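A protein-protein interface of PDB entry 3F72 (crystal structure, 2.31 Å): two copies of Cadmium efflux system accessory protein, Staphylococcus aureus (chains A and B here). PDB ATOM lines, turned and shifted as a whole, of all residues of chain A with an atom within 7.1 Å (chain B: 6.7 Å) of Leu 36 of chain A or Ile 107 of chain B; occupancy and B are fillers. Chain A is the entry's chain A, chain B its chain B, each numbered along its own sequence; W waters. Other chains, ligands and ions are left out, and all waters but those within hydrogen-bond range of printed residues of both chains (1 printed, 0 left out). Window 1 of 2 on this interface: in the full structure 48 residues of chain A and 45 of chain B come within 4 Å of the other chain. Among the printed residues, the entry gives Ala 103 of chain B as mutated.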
ATOM      1  N   GLY A  31      20.645   9.646 -13.075  1.00  0.00           N
ATOM      2  CA  GLY A  31      20.429   8.470 -12.300  1.00  0.00           C
ATOM      3  C   GLY A  31      20.548   7.212 -13.120  1.00  0.00           C
ATOM      4  O   GLY A  31      21.047   6.253 -12.629  1.00  0.00           O
ATOM      5  N   VAL A  32      20.185   7.169 -14.382  1.00  0.00           N
ATOM      6  CA  VAL A  32      20.430   5.932 -15.134  1.00  0.00           C
ATOM      7  C   VAL A  32      21.820   5.596 -15.517  1.00  0.00           C
ATOM      8  O   VAL A  32      22.182   4.401 -15.537  1.00  0.00           O
ATOM      9  CB  VAL A  32      19.544   5.986 -16.341  1.00  0.00           C
ATOM     10  CG1 VAL A  32      20.182   6.668 -17.516  1.00  0.00           C
ATOM     11  CG2 VAL A  32      19.117   4.651 -16.667  1.00  0.00           C
ATOM     12  N   SER A  33      22.641   6.631 -15.869  1.00  0.00           N
ATOM     13  CA  SER A  33      24.083   6.519 -16.028  1.00  0.00           C
ATOM     14  C   SER A  33      24.721   6.043 -14.747  1.00  0.00           C
ATOM     15  O   SER A  33      25.610   5.213 -14.862  1.00  0.00           O
ATOM     16  CB  SER A  33      24.744   7.893 -16.280  1.00  0.00           C
ATOM     17  OG  SER A  33      24.009   8.576 -17.262  1.00  0.00           O
ATOM     18  N   GLN A  34      24.307   6.563 -13.590  1.00  0.00           N
ATOM     19  CA  GLN A  34      24.808   6.007 -12.302  1.00  0.00           C
ATOM     20  C   GLN A  34      24.573   4.499 -12.149  1.00  0.00           C
ATOM     21  O   GLN A  34      25.518   3.803 -11.924  1.00  0.00           O
ATOM     22  CB  GLN A  34      24.300   6.748 -11.068  1.00  0.00           C
ATOM     23  CG  GLN A  34      24.889   8.149 -10.895  1.00  0.00           C
ATOM     24  CD  GLN A  34      24.253   8.976  -9.686  1.00  0.00           C
ATOM     25  OE1 GLN A  34      23.417   9.898  -9.876  1.00  0.00           O
ATOM     26  NE2 GLN A  34      24.666   8.629  -8.443  1.00  0.00           N
ATOM     27  N   ILE A  35      23.327   4.008 -12.322  1.00  0.00           N
ATOM     28  CA  ILE A  35      23.031   2.625 -12.176  1.00  0.00           C
ATOM     29  C   ILE A  35      23.683   1.745 -13.203  1.00  0.00           C
ATOM     30  O   ILE A  35      24.384   0.721 -12.853  1.00  0.00           O
ATOM     31  CB  ILE A  35      21.622   2.392 -11.905  1.00  0.00           C
ATOM     32  CG1 ILE A  35      21.556   1.048 -11.184  1.00  0.00           C
ATOM     33  CG2 ILE A  35      20.807   2.401 -13.175  1.00  0.00           C
ATOM     34  CD1 ILE A  35      20.077   0.449 -10.963  1.00  0.00           C
ATOM     35  N   LEU A  36      23.670   2.182 -14.480  1.00  0.00           N
ATOM     36  CA  LEU A  36      24.404   1.399 -15.470  1.00  0.00           C
ATOM     37  C   LEU A  36      25.874   1.438 -15.242  1.00  0.00           C
ATOM     38  O   LEU A  36      26.556   0.489 -15.590  1.00  0.00           O
ATOM     39  CB  LEU A  36      24.026   1.736 -16.915  1.00  0.00           C
ATOM     40  CG  LEU A  36      22.498   1.618 -17.218  1.00  0.00           C
ATOM     41  CD1 LEU A  36      22.008   2.277 -18.533  1.00  0.00           C
ATOM     42  CD2 LEU A  36      21.972   0.198 -17.109  1.00  0.00           C
ATOM     43  N   LYS A  37      26.398   2.503 -14.657  1.00  0.00           N
ATOM     44  CA  LYS A  37      27.900   2.538 -14.366  1.00  0.00           C
ATOM     45  C   LYS A  37      28.277   1.564 -13.220  1.00  0.00           C
ATOM     46  O   LYS A  37      29.313   0.855 -13.284  1.00  0.00           O
ATOM     47  CB  LYS A  37      28.398   3.940 -13.969  1.00  0.00           C
ATOM     48  CG  LYS A  37      28.913   4.730 -15.101  1.00  0.00           C
ATOM     49  CD  LYS A  37      29.343   6.130 -14.730  1.00  0.00           C
ATOM     50  CE  LYS A  37      29.350   7.163 -16.020  1.00  0.00           C
ATOM     51  NZ  LYS A  37      29.798   6.468 -17.291  1.00  0.00           N
ATOM     52  N   ALA A  38      27.395   1.499 -12.215  1.00  0.00           N
ATOM     53  CA  ALA A  38      27.560   0.512 -11.132  1.00  0.00           C
ATOM     54  C   ALA A  38      27.654  -0.861 -11.696  1.00  0.00           C
ATOM     55  O   ALA A  38      28.655  -1.530 -11.434  1.00  0.00           O
ATOM     56  CB  ALA A  38      26.414   0.550 -10.152  1.00  0.00           C
ATOM     57  N   ILE A  39      26.629  -1.303 -12.454  1.00  0.00           N
ATOM     58  CA  ILE A  39      26.645  -2.616 -13.100  1.00  0.00           C
ATOM     59  C   ILE A  39      27.729  -2.911 -14.129  1.00  0.00           C
ATOM     60  O   ILE A  39      28.139  -4.072 -14.250  1.00  0.00           O
ATOM     61  CB  ILE A  39      25.322  -3.030 -13.700  1.00  0.00           C
ATOM     62  CG1 ILE A  39      24.229  -2.771 -12.755  1.00  0.00           C
ATOM     63  CG2 ILE A  39      25.360  -4.455 -13.924  1.00  0.00           C
ATOM     64  CD1 ILE A  39      22.917  -2.851 -13.404  1.00  0.00           C
ATOM     65  N   ALA A  40      28.207  -1.911 -14.853  1.00  0.00           N
ATOM     66  CA  ALA A  40      29.015  -2.158 -16.054  1.00  0.00           C
ATOM     67  C   ALA A  40      30.405  -2.663 -15.731  1.00  0.00           C
ATOM     68  O   ALA A  40      31.111  -3.266 -16.547  1.00  0.00           O
ATOM     69  CB  ALA A  40      29.115  -0.912 -16.906  1.00  0.00           C
ATOM     70  N   ASP A  41      30.858  -2.333 -14.564  1.00  0.00           N
ATOM     71  CA  ASP A  41      32.204  -2.648 -14.183  1.00  0.00           C
ATOM     72  C   ASP A  41      32.411  -4.164 -14.297  1.00  0.00           C
ATOM     73  O   ASP A  41      31.570  -4.910 -13.908  1.00  0.00           O
ATOM     74  CB  ASP A  41      32.329  -2.244 -12.712  1.00  0.00           C
ATOM     75  CG  ASP A  41      33.528  -2.916 -12.015  1.00  0.00           C
ATOM     76  OD1 ASP A  41      34.602  -2.304 -12.132  1.00  0.00           O
ATOM     77  OD2 ASP A  41      33.365  -4.042 -11.394  1.00  0.00           O
ATOM     78  N   GLN A  83      23.193   2.179  -5.433  1.00  0.00           N
ATOM     79  CA  GLN A  83      22.391   2.320  -6.647  1.00  0.00           C
ATOM     80  C   GLN A  83      21.174   1.419  -6.630  1.00  0.00           C
ATOM     81  O   GLN A  83      20.305   1.528  -7.535  1.00  0.00           O
ATOM     82  CB  GLN A  83      23.179   2.053  -7.900  1.00  0.00           C
ATOM     83  CG  GLN A  83      24.298   2.955  -8.149  1.00  0.00           C
ATOM     84  CD  GLN A  83      23.923   4.406  -8.100  1.00  0.00           C
ATOM     85  OE1 GLN A  83      22.758   4.756  -8.399  1.00  0.00           O
ATOM     86  NE2 GLN A  83      24.912   5.285  -7.760  1.00  0.00           N
ATOM     87  N   VAL A  85      21.253  -1.774  -6.914  1.00  0.00           N
ATOM     88  CA  VAL A  85      21.510  -3.017  -7.653  1.00  0.00           C
ATOM     89  C   VAL A  85      21.458  -4.219  -6.691  1.00  0.00           C
ATOM     90  O   VAL A  85      20.940  -5.322  -7.046  1.00  0.00           O
ATOM     91  CB  VAL A  85      22.789  -2.877  -8.500  1.00  0.00           C
ATOM     92  CG1 VAL A  85      23.043  -4.057  -9.414  1.00  0.00           C
ATOM     93  CG2 VAL A  85      22.698  -1.637  -9.361  1.00  0.00           C
ATOM     94  N   GLN A 106      16.290  -8.616 -15.036  1.00  0.00           N
ATOM     95  CA  GLN A 106      15.949  -8.304 -16.424  1.00  0.00           C
ATOM     96  C   GLN A 106      17.132  -7.628 -17.139  1.00  0.00           C
ATOM     97  O   GLN A 106      17.511  -8.012 -18.250  1.00  0.00           O
ATOM     98  CB  GLN A 106      14.670  -7.455 -16.529  1.00  0.00           C
ATOM     99  CG  GLN A 106      13.458  -8.034 -15.942  1.00  0.00           C
ATOM    100  CD  GLN A 106      13.381  -9.424 -16.390  1.00  0.00           C
ATOM    101  OE1 GLN A 106      13.542 -10.350 -15.589  1.00  0.00           O
ATOM    102  NE2 GLN A 106      13.218  -9.629 -17.728  1.00  0.00           N
ATOM    103  N   ILE A 107      17.715  -6.619 -16.513  1.00  0.00           N
ATOM    104  CA  ILE A 107      18.757  -5.846 -17.156  1.00  0.00           C
ATOM    105  C   ILE A 107      19.859  -6.788 -17.647  1.00  0.00           C
ATOM    106  O   ILE A 107      20.229  -6.793 -18.787  1.00  0.00           O
ATOM    107  CB  ILE A 107      19.250  -4.650 -16.265  1.00  0.00           C
ATOM    108  CG1 ILE A 107      18.197  -3.525 -16.254  1.00  0.00           C
ATOM    109  CG2 ILE A 107      20.527  -4.127 -16.774  1.00  0.00           C
ATOM    110  CD1 ILE A 107      18.433  -2.450 -15.271  1.00  0.00           C
ATOM    111  N   MET A 108      20.319  -7.648 -16.781  1.00  0.00           N
ATOM    112  CA  MET A 108      21.392  -8.597 -17.064  1.00  0.00           C
ATOM    113  C   MET A 108      20.998  -9.658 -18.102  1.00  0.00           C
ATOM    114  O   MET A 108      21.783 -10.082 -18.959  1.00  0.00           O
ATOM    115  CB  MET A 108      21.654  -9.368 -15.747  1.00  0.00           C
ATOM    116  CG  MET A 108      22.719 -10.468 -15.930  1.00  0.00           C
ATOM    117  SD  MET A 108      24.284  -9.562 -16.023  1.00  0.00           S
ATOM    118  CE  MET A 108      24.763 -10.302 -17.501  1.00  0.00           C
ATOM    119  N   ILE A 110      18.473  -9.660 -20.399  1.00  0.00           N
ATOM    120  CA  ILE A 110      18.287  -8.989 -21.700  1.00  0.00           C
ATOM    121  C   ILE A 110      19.615  -8.627 -22.353  1.00  0.00           C
ATOM    122  O   ILE A 110      19.884  -8.944 -23.533  1.00  0.00           O
ATOM    123  CB  ILE A 110      17.378  -7.736 -21.544  1.00  0.00           C
ATOM    124  CG1 ILE A 110      15.982  -8.172 -21.013  1.00  0.00           C
ATOM    125  CG2 ILE A 110      17.283  -6.968 -22.884  1.00  0.00           C
ATOM    126  CD1 ILE A 110      15.002  -7.097 -20.447  1.00  0.00           C
ATOM    127  N   ALA A 111      20.487  -8.030 -21.565  1.00  0.00           N
ATOM    128  CA  ALA A 111      21.871  -7.732 -21.951  1.00  0.00           C
ATOM    129  C   ALA A 111      22.553  -8.983 -22.479  1.00  0.00           C
ATOM    130  O   ALA A 111      22.889  -9.068 -23.656  1.00  0.00           O
ATOM    131  CB  ALA A 111      22.620  -7.083 -20.732  1.00  0.00           C
ATOM    132  N   LEU A 112      22.666 -10.003 -21.639  1.00  0.00           N
ATOM    133  CA  LEU A 112      23.028 -11.384 -22.085  1.00  0.00           C
ATOM    134  C   LEU A 112      22.448 -11.855 -23.467  1.00  0.00           C
ATOM    135  O   LEU A 112      23.188 -12.039 -24.436  1.00  0.00           O
ATOM    136  CB  LEU A 112      22.665 -12.374 -20.985  1.00  0.00           C
ATOM    137  CG  LEU A 112      23.517 -12.286 -19.732  1.00  0.00           C
ATOM    138  CD1 LEU A 112      22.974 -13.256 -18.740  1.00  0.00           C
ATOM    139  CD2 LEU A 112      24.895 -12.657 -20.026  1.00  0.00           C
ATOM    140  N   HIS A 114      20.809 -10.066 -25.804  1.00  0.00           N
ATOM    141  CA  HIS A 114      21.270  -9.184 -26.898  1.00  0.00           C
ATOM    142  C   HIS A 114      22.626  -9.552 -27.560  1.00  0.00           C
ATOM    143  O   HIS A 114      22.726  -9.705 -28.781  1.00  0.00           O
ATOM    144  CB  HIS A 114      21.371  -7.753 -26.392  1.00  0.00           C
ATOM    145  CG  HIS A 114      21.721  -6.764 -27.447  1.00  0.00           C
ATOM    146  ND1 HIS A 114      20.882  -6.473 -28.505  1.00  0.00           N
ATOM    147  CD2 HIS A 114      22.807  -5.976 -27.603  1.00  0.00           C
ATOM    148  CE1 HIS A 114      21.440  -5.554 -29.267  1.00  0.00           C
ATOM    149  NE2 HIS A 114      22.595  -5.218 -28.732  1.00  0.00           N
ATOM    150  N   SER B  33      29.189  -6.045 -19.912  1.00  0.00           N
ATOM    151  CA  SER B  33      29.835  -4.970 -19.281  1.00  0.00           C
ATOM    152  C   SER B  33      30.270  -3.943 -20.325  1.00  0.00           C
ATOM    153  O   SER B  33      30.252  -2.682 -20.105  1.00  0.00           O
ATOM    154  CB  SER B  33      30.914  -5.612 -18.356  1.00  0.00           C
ATOM    155  OG  SER B  33      32.046  -4.838 -18.217  1.00  0.00           O
ATOM    156  N   ILE B  35      28.626  -3.279 -23.260  1.00  0.00           N
ATOM    157  CA  ILE B  35      27.369  -2.701 -23.658  1.00  0.00           C
ATOM    158  C   ILE B  35      26.900  -1.752 -22.639  1.00  0.00           C
ATOM    159  O   ILE B  35      26.570  -0.646 -22.984  1.00  0.00           O
ATOM    160  CB  ILE B  35      26.262  -3.808 -24.080  1.00  0.00           C
ATOM    161  CG1 ILE B  35      26.871  -4.743 -25.078  1.00  0.00           C
ATOM    162  CG2 ILE B  35      25.153  -3.306 -24.978  1.00  0.00           C
ATOM    163  CD1 ILE B  35      28.006  -4.088 -26.180  1.00  0.00           C
ATOM    164  N   LEU B  36      26.814  -2.128 -21.395  1.00  0.00           N
ATOM    165  CA  LEU B  36      26.322  -1.163 -20.360  1.00  0.00           C
ATOM    166  C   LEU B  36      27.239   0.075 -20.258  1.00  0.00           C
ATOM    167  O   LEU B  36      26.759   1.224 -19.973  1.00  0.00           O
ATOM    168  CB  LEU B  36      26.266  -1.896 -19.029  1.00  0.00           C
ATOM    169  CG  LEU B  36      25.209  -3.020 -19.010  1.00  0.00           C
ATOM    170  CD1 LEU B  36      25.066  -3.631 -17.625  1.00  0.00           C
ATOM    171  CD2 LEU B  36      23.768  -2.601 -19.731  1.00  0.00           C
ATOM    172  N   LYS B  37      28.554  -0.142 -20.479  1.00  0.00           N
ATOM    173  CA  LYS B  37      29.567   0.935 -20.420  1.00  0.00           C
ATOM    174  C   LYS B  37      29.338   1.864 -21.543  1.00  0.00           C
ATOM    175  O   LYS B  37      29.384   3.077 -21.435  1.00  0.00           O
ATOM    176  CB  LYS B  37      30.977   0.344 -20.525  1.00  0.00           C
ATOM    177  CG  LYS B  37      32.051   1.231 -19.931  1.00  0.00           C
ATOM    178  CD  LYS B  37      33.462   1.151 -20.680  1.00  0.00           C
ATOM    179  CE  LYS B  37      34.337   2.536 -20.545  1.00  0.00           C
ATOM    180  NZ  LYS B  37      33.738   3.994 -20.940  1.00  0.00           N
ATOM    181  N   ILE B  39      26.376   2.387 -22.971  1.00  0.00           N
ATOM    182  CA  ILE B  39      25.170   3.113 -22.698  1.00  0.00           C
ATOM    183  C   ILE B  39      25.347   4.104 -21.506  1.00  0.00           C
ATOM    184  O   ILE B  39      24.826   5.231 -21.498  1.00  0.00           O
ATOM    185  CB  ILE B  39      24.106   2.072 -22.349  1.00  0.00           C
ATOM    186  CG1 ILE B  39      23.671   1.332 -23.572  1.00  0.00           C
ATOM    187  CG2 ILE B  39      22.893   2.764 -21.749  1.00  0.00           C
ATOM    188  CD1 ILE B  39      22.769   0.066 -23.262  1.00  0.00           C
ATOM    189  N   ALA B  40      26.108   3.695 -20.493  1.00  0.00           N
ATOM    190  CA  ALA B  40      26.116   4.436 -19.250  1.00  0.00           C
ATOM    191  C   ALA B  40      26.632   5.913 -19.227  1.00  0.00           C
ATOM    192  O   ALA B  40      26.286   6.651 -18.355  1.00  0.00           O
ATOM    193  CB  ALA B  40      26.760   3.605 -18.206  1.00  0.00           C
ATOM    194  N   ASP B  41      27.396   6.390 -20.193  1.00  0.00           N
ATOM    195  CA  ASP B  41      27.828   7.723 -20.164  1.00  0.00           C
ATOM    196  C   ASP B  41      26.654   8.585 -20.461  1.00  0.00           C
ATOM    197  O   ASP B  41      25.961   8.399 -21.425  1.00  0.00           O
ATOM    198  CB  ASP B  41      28.950   7.889 -21.194  1.00  0.00           C
ATOM    199  CG  ASP B  41      29.167   9.340 -21.643  1.00  0.00           C
ATOM    200  OD1 ASP B  41      28.384   9.972 -22.385  1.00  0.00           O
ATOM    201  OD2 ASP B  41      30.229   9.869 -21.296  1.00  0.00           O
ATOM    202  N   ALA B  45      23.729   8.024 -22.994  1.00  0.00           N
ATOM    203  CA  ALA B  45      22.503   7.621 -22.317  1.00  0.00           C
ATOM    204  C   ALA B  45      21.341   8.505 -22.743  1.00  0.00           C
ATOM    205  O   ALA B  45      20.251   8.035 -22.872  1.00  0.00           O
ATOM    206  CB  ALA B  45      22.632   7.640 -20.823  1.00  0.00           C
ATOM    207  N   GLU B 102      15.451  -3.830 -29.732  1.00  0.00           N
ATOM    208  CA  GLU B 102      14.480  -3.672 -28.623  1.00  0.00           C
ATOM    209  C   GLU B 102      15.060  -3.908 -27.223  1.00  0.00           C
ATOM    210  O   GLU B 102      14.679  -3.270 -26.259  1.00  0.00           O
ATOM    211  CB  GLU B 102      13.269  -4.644 -28.884  1.00  0.00           C
ATOM    212  CG  GLU B 102      12.267  -4.085 -29.899  1.00  0.00           C
ATOM    213  CD  GLU B 102      11.950  -2.640 -29.683  1.00  0.00           C
ATOM    214  OE1 GLU B 102      11.250  -2.250 -28.636  1.00  0.00           O
ATOM    215  OE2 GLU B 102      12.379  -1.891 -30.624  1.00  0.00           O
ATOM    216  N   ALA B 103      16.015  -4.774 -27.144  1.00  0.00           N
ATOM    217  CA  ALA B 103      16.765  -5.035 -25.965  1.00  0.00           C
ATOM    218  C   ALA B 103      17.402  -3.736 -25.425  1.00  0.00           C
ATOM    219  O   ALA B 103      17.583  -3.522 -24.173  1.00  0.00           O
ATOM    220  CB  ALA B 103      17.775  -5.976 -26.287  1.00  0.00           C
ATOM    221  N   ILE B 104      17.657  -2.792 -26.325  1.00  0.00           N
ATOM    222  CA  ILE B 104      18.325  -1.628 -25.846  1.00  0.00           C
ATOM    223  C   ILE B 104      17.275  -0.720 -25.332  1.00  0.00           C
ATOM    224  O   ILE B 104      17.471  -0.098 -24.302  1.00  0.00           O
ATOM    225  CB  ILE B 104      19.190  -1.036 -26.925  1.00  0.00           C
ATOM    226  CG1 ILE B 104      20.431  -1.906 -26.994  1.00  0.00           C
ATOM    227  CG2 ILE B 104      19.620   0.291 -26.484  1.00  0.00           C
ATOM    228  CD1 ILE B 104      20.652  -2.248 -28.344  1.00  0.00           C
ATOM    229  N   ARG B 105      16.102  -0.711 -25.961  1.00  0.00           N
ATOM    230  CA  ARG B 105      14.940   0.008 -25.316  1.00  0.00           C
ATOM    231  C   ARG B 105      14.626  -0.458 -23.858  1.00  0.00           C
ATOM    232  O   ARG B 105      14.497   0.296 -22.943  1.00  0.00           O
ATOM    233  CB  ARG B 105      13.686  -0.090 -26.171  1.00  0.00           C
ATOM    234  CG  ARG B 105      12.504   0.619 -25.525  1.00  0.00           C
ATOM    235  CD  ARG B 105      11.157   0.301 -26.300  1.00  0.00           C
ATOM    236  NE  ARG B 105      11.429   0.532 -27.715  1.00  0.00           N
ATOM    237  CZ  ARG B 105      11.389   1.746 -28.296  1.00  0.00           C
ATOM    238  NH1 ARG B 105      11.060   2.866 -27.614  1.00  0.00           N
ATOM    239  NH2 ARG B 105      11.781   1.839 -29.550  1.00  0.00           N
ATOM    240  N   GLN B 106      14.568  -1.734 -23.695  1.00  0.00           N
ATOM    241  CA  GLN B 106      14.269  -2.322 -22.427  1.00  0.00           C
ATOM    242  C   GLN B 106      15.279  -2.147 -21.325  1.00  0.00           C
ATOM    243  O   GLN B 106      14.831  -1.950 -20.164  1.00  0.00           O
ATOM    244  CB  GLN B 106      14.039  -3.788 -22.627  1.00  0.00           C
ATOM    245  CG  GLN B 106      12.602  -4.006 -23.121  1.00  0.00           C
ATOM    246  CD  GLN B 106      12.403  -5.479 -23.211  1.00  0.00           C
ATOM    247  OE1 GLN B 106      11.943  -6.139 -22.229  1.00  0.00           O
ATOM    248  NE2 GLN B 106      12.879  -6.052 -24.312  1.00  0.00           N
ATOM    249  N   ILE B 107      16.603  -2.136 -21.634  1.00  0.00           N
ATOM    250  CA  ILE B 107      17.562  -1.912 -20.579  1.00  0.00           C
ATOM    251  C   ILE B 107      17.423  -0.499 -20.053  1.00  0.00           C
ATOM    252  O   ILE B 107      17.549  -0.257 -18.876  1.00  0.00           O
ATOM    253  CB  ILE B 107      19.025  -2.166 -21.057  1.00  0.00           C
ATOM    254  CG1 ILE B 107      19.229  -3.669 -21.322  1.00  0.00           C
ATOM    255  CG2 ILE B 107      20.015  -1.621 -20.005  1.00  0.00           C
ATOM    256  CD1 ILE B 107      20.439  -3.967 -22.259  1.00  0.00           C
ATOM    257  N   MET B 108      17.171   0.430 -20.934  1.00  0.00           N
ATOM    258  CA  MET B 108      17.114   1.814 -20.585  1.00  0.00           C
ATOM    259  C   MET B 108      15.847   2.071 -19.792  1.00  0.00           C
ATOM    260  O   MET B 108      15.861   2.669 -18.687  1.00  0.00           O
ATOM    261  CB  MET B 108      17.187   2.711 -21.881  1.00  0.00           C
ATOM    262  CG  MET B 108      16.730   4.115 -21.625  1.00  0.00           C
ATOM    263  SD  MET B 108      17.864   5.153 -20.676  1.00  0.00           S
ATOM    264  CE  MET B 108      19.341   4.965 -21.633  1.00  0.00           C
ATOM    265  N   MET B 109      14.748   1.656 -20.362  1.00  0.00           N
ATOM    266  CA  MET B 109      13.428   1.751 -19.682  1.00  0.00           C
ATOM    267  C   MET B 109      13.377   1.005 -18.356  1.00  0.00           C
ATOM    268  O   MET B 109      12.926   1.592 -17.366  1.00  0.00           O
ATOM    269  CB  MET B 109      12.245   1.392 -20.664  1.00  0.00           C
ATOM    270  CG  MET B 109      11.326   2.756 -21.083  1.00  0.00           C
ATOM    271  SD  MET B 109      12.436   4.096 -21.796  1.00  0.00           S
ATOM    272  CE  MET B 109      11.207   5.319 -22.327  1.00  0.00           C
ATOM    273  N   ILE B 110      13.819  -0.249 -18.290  1.00  0.00           N
ATOM    274  CA  ILE B 110      13.863  -0.894 -16.929  1.00  0.00           C
ATOM    275  C   ILE B 110      14.794  -0.108 -15.920  1.00  0.00           C
ATOM    276  O   ILE B 110      14.445   0.096 -14.743  1.00  0.00           O
ATOM    277  CB  ILE B 110      14.284  -2.475 -16.957  1.00  0.00           C
ATOM    278  CG1 ILE B 110      13.547  -3.315 -17.981  1.00  0.00           C
ATOM    279  CG2 ILE B 110      14.350  -3.126 -15.524  1.00  0.00           C
ATOM    280  CD1 ILE B 110      12.266  -2.848 -18.162  1.00  0.00           C
ATOM    281  N   ALA B 111      15.951   0.353 -16.394  1.00  0.00           N
ATOM    282  CA  ALA B 111      16.852   1.130 -15.490  1.00  0.00           C
ATOM    283  C   ALA B 111      16.276   2.441 -15.035  1.00  0.00           C
ATOM    284  O   ALA B 111      16.452   2.852 -13.862  1.00  0.00           O
ATOM    285  CB  ALA B 111      18.253   1.350 -16.130  1.00  0.00           C
ATOM    286  N   LEU B 112      15.599   3.125 -15.950  1.00  0.00           N
ATOM    287  CA  LEU B 112      14.848   4.317 -15.535  1.00  0.00           C
ATOM    288  C   LEU B 112      13.710   4.063 -14.477  1.00  0.00           C
ATOM    289  O   LEU B 112      13.497   4.867 -13.537  1.00  0.00           O
ATOM    290  CB  LEU B 112      14.291   5.055 -16.743  1.00  0.00           C
ATOM    291  CG  LEU B 112      15.284   5.875 -17.558  1.00  0.00           C
ATOM    292  CD1 LEU B 112      14.573   6.134 -18.844  1.00  0.00           C
ATOM    293  CD2 LEU B 112      15.586   7.157 -16.862  1.00  0.00           C
HETATM  294  O   HOH W   1      30.367   4.301 -19.146  1.00  0.00           O
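Of the printed residues of chain B, Leu 36 of chain A touches Ile 39 (3.4 Å), Ala 40 (3.6 Å) and Ile 107 (3.9 Å). Of the printed residues of chain B, Ile 110 of chain A touches Ala 103 and Gln 106. Of the printed residues of chain A, Gln 106 of chain B touches Ile 110 (3.7 Å). Ile 107 of chain B touches just one residue of chain A: Leu 36.
Printed residues of chain A that touch a printed residue of chain B: Val 32, Ser 33, Leu 36, Lys 37, Ile 39, Ala 40, Asp 41, Ile 107, Ile 110 and His 114. Hydrophobic or aromatic side chains of chain A that line the printed part of chain B: Val 32, Leu 36, Ile 39, Ala 40, Ile 107, Ile 110 and His 114. Of the 19 printed residues of chain B, 14 touch a printed residue of chain A. Printed residues of chain B that touch a printed residue of chain A: Ser 33, Leu 36, Lys 37, Ile 39, Ala 40, Asp 41, Ala 45, Ala 103, Ile 104, Gln 106, Ile 107, Ile 110, Ala 111 and Leu 112. Hydrophobic or aromatic side chains of chain B that line the printed part of chain A: Leu 36, Ile 39, Ala 40, Ala 45, Ala 103, Ile 104, Ile 107, Ile 110 and Ala 111.
The backbone carbonyl oxygen (O) of Ile 39 of chain B lies close to the backbone NH (N) of Ala 45 of chain B (3.4 Å).
The backbone carbonyl oxygen of Ala 40 of chain A sits at hydrogen-bond distance from the side-chain hydroxyl of Ser 33 of chain B (2.5 Å). O of Ala 40 of chain B lies close to OG of Ser 33 of chain A (3.2 Å).
Water W1 lies within hydrogen-bond range of the backbone carbonyl oxygen of Lys 37 of chain B and the side-chain amino group of Lys 37 of chain A.
Ala 45 of chain B touches Ser 33 of chain A (CB to OG, 3.9 Å). CB of Ala 40 of chain B touches CB of Leu 36 of chain A, at 3.6 Å. Ala 40 of chain B touches Lys 37 of chain A (O to NZ, 3.7 Å). Lys 37 of chain A touches Asp 41 of chain B (NZ to CA, 3.7 Å). CG2 of Ile 39 of chain A touches CD1 of Leu 36 of chain B (3.8 Å). Ala 40 of chain A touches Leu 36 of chain B (CB to CB, 3.7 Å). Ile 107 of chain A touches Ile 110 of chain B. CD1 of Ile 107 of chain A touches CB of Ala 111 of chain B, 3.9 Å away. His 114 of chain A touches Ala 103 of chain B (ND1 to CB, 3.8 Å). Ile 104 of chain B touches His 114 of chain A.
Leu 36 of chain A touches Ala 40 of chain B, and with the chains exchanged Ala 40 of chain A touches Leu 36 of chain B. Leu 36 of chain A touches Ile 107 of chain B, but with the chains exchanged Ile 107 of chain A does not touch Leu 36 of chain B (4.6 Å). Lys 37 of chain A touches Asp 41 of chain B, but with the chains exchanged Asp 41 of chain A does not touch Lys 37 of chain B (6.5 Å). Ile 110 of chain A touches Gln 106 of chain B, but with the chains exchanged Gln 106 of chain A does not touch Ile 110 of chain B (4.5 Å). 13 positions are printed for both chains. Of the 20 pairs that touch across the chains among the printed residues, 8 have their exchanged pair printed and touching as well.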
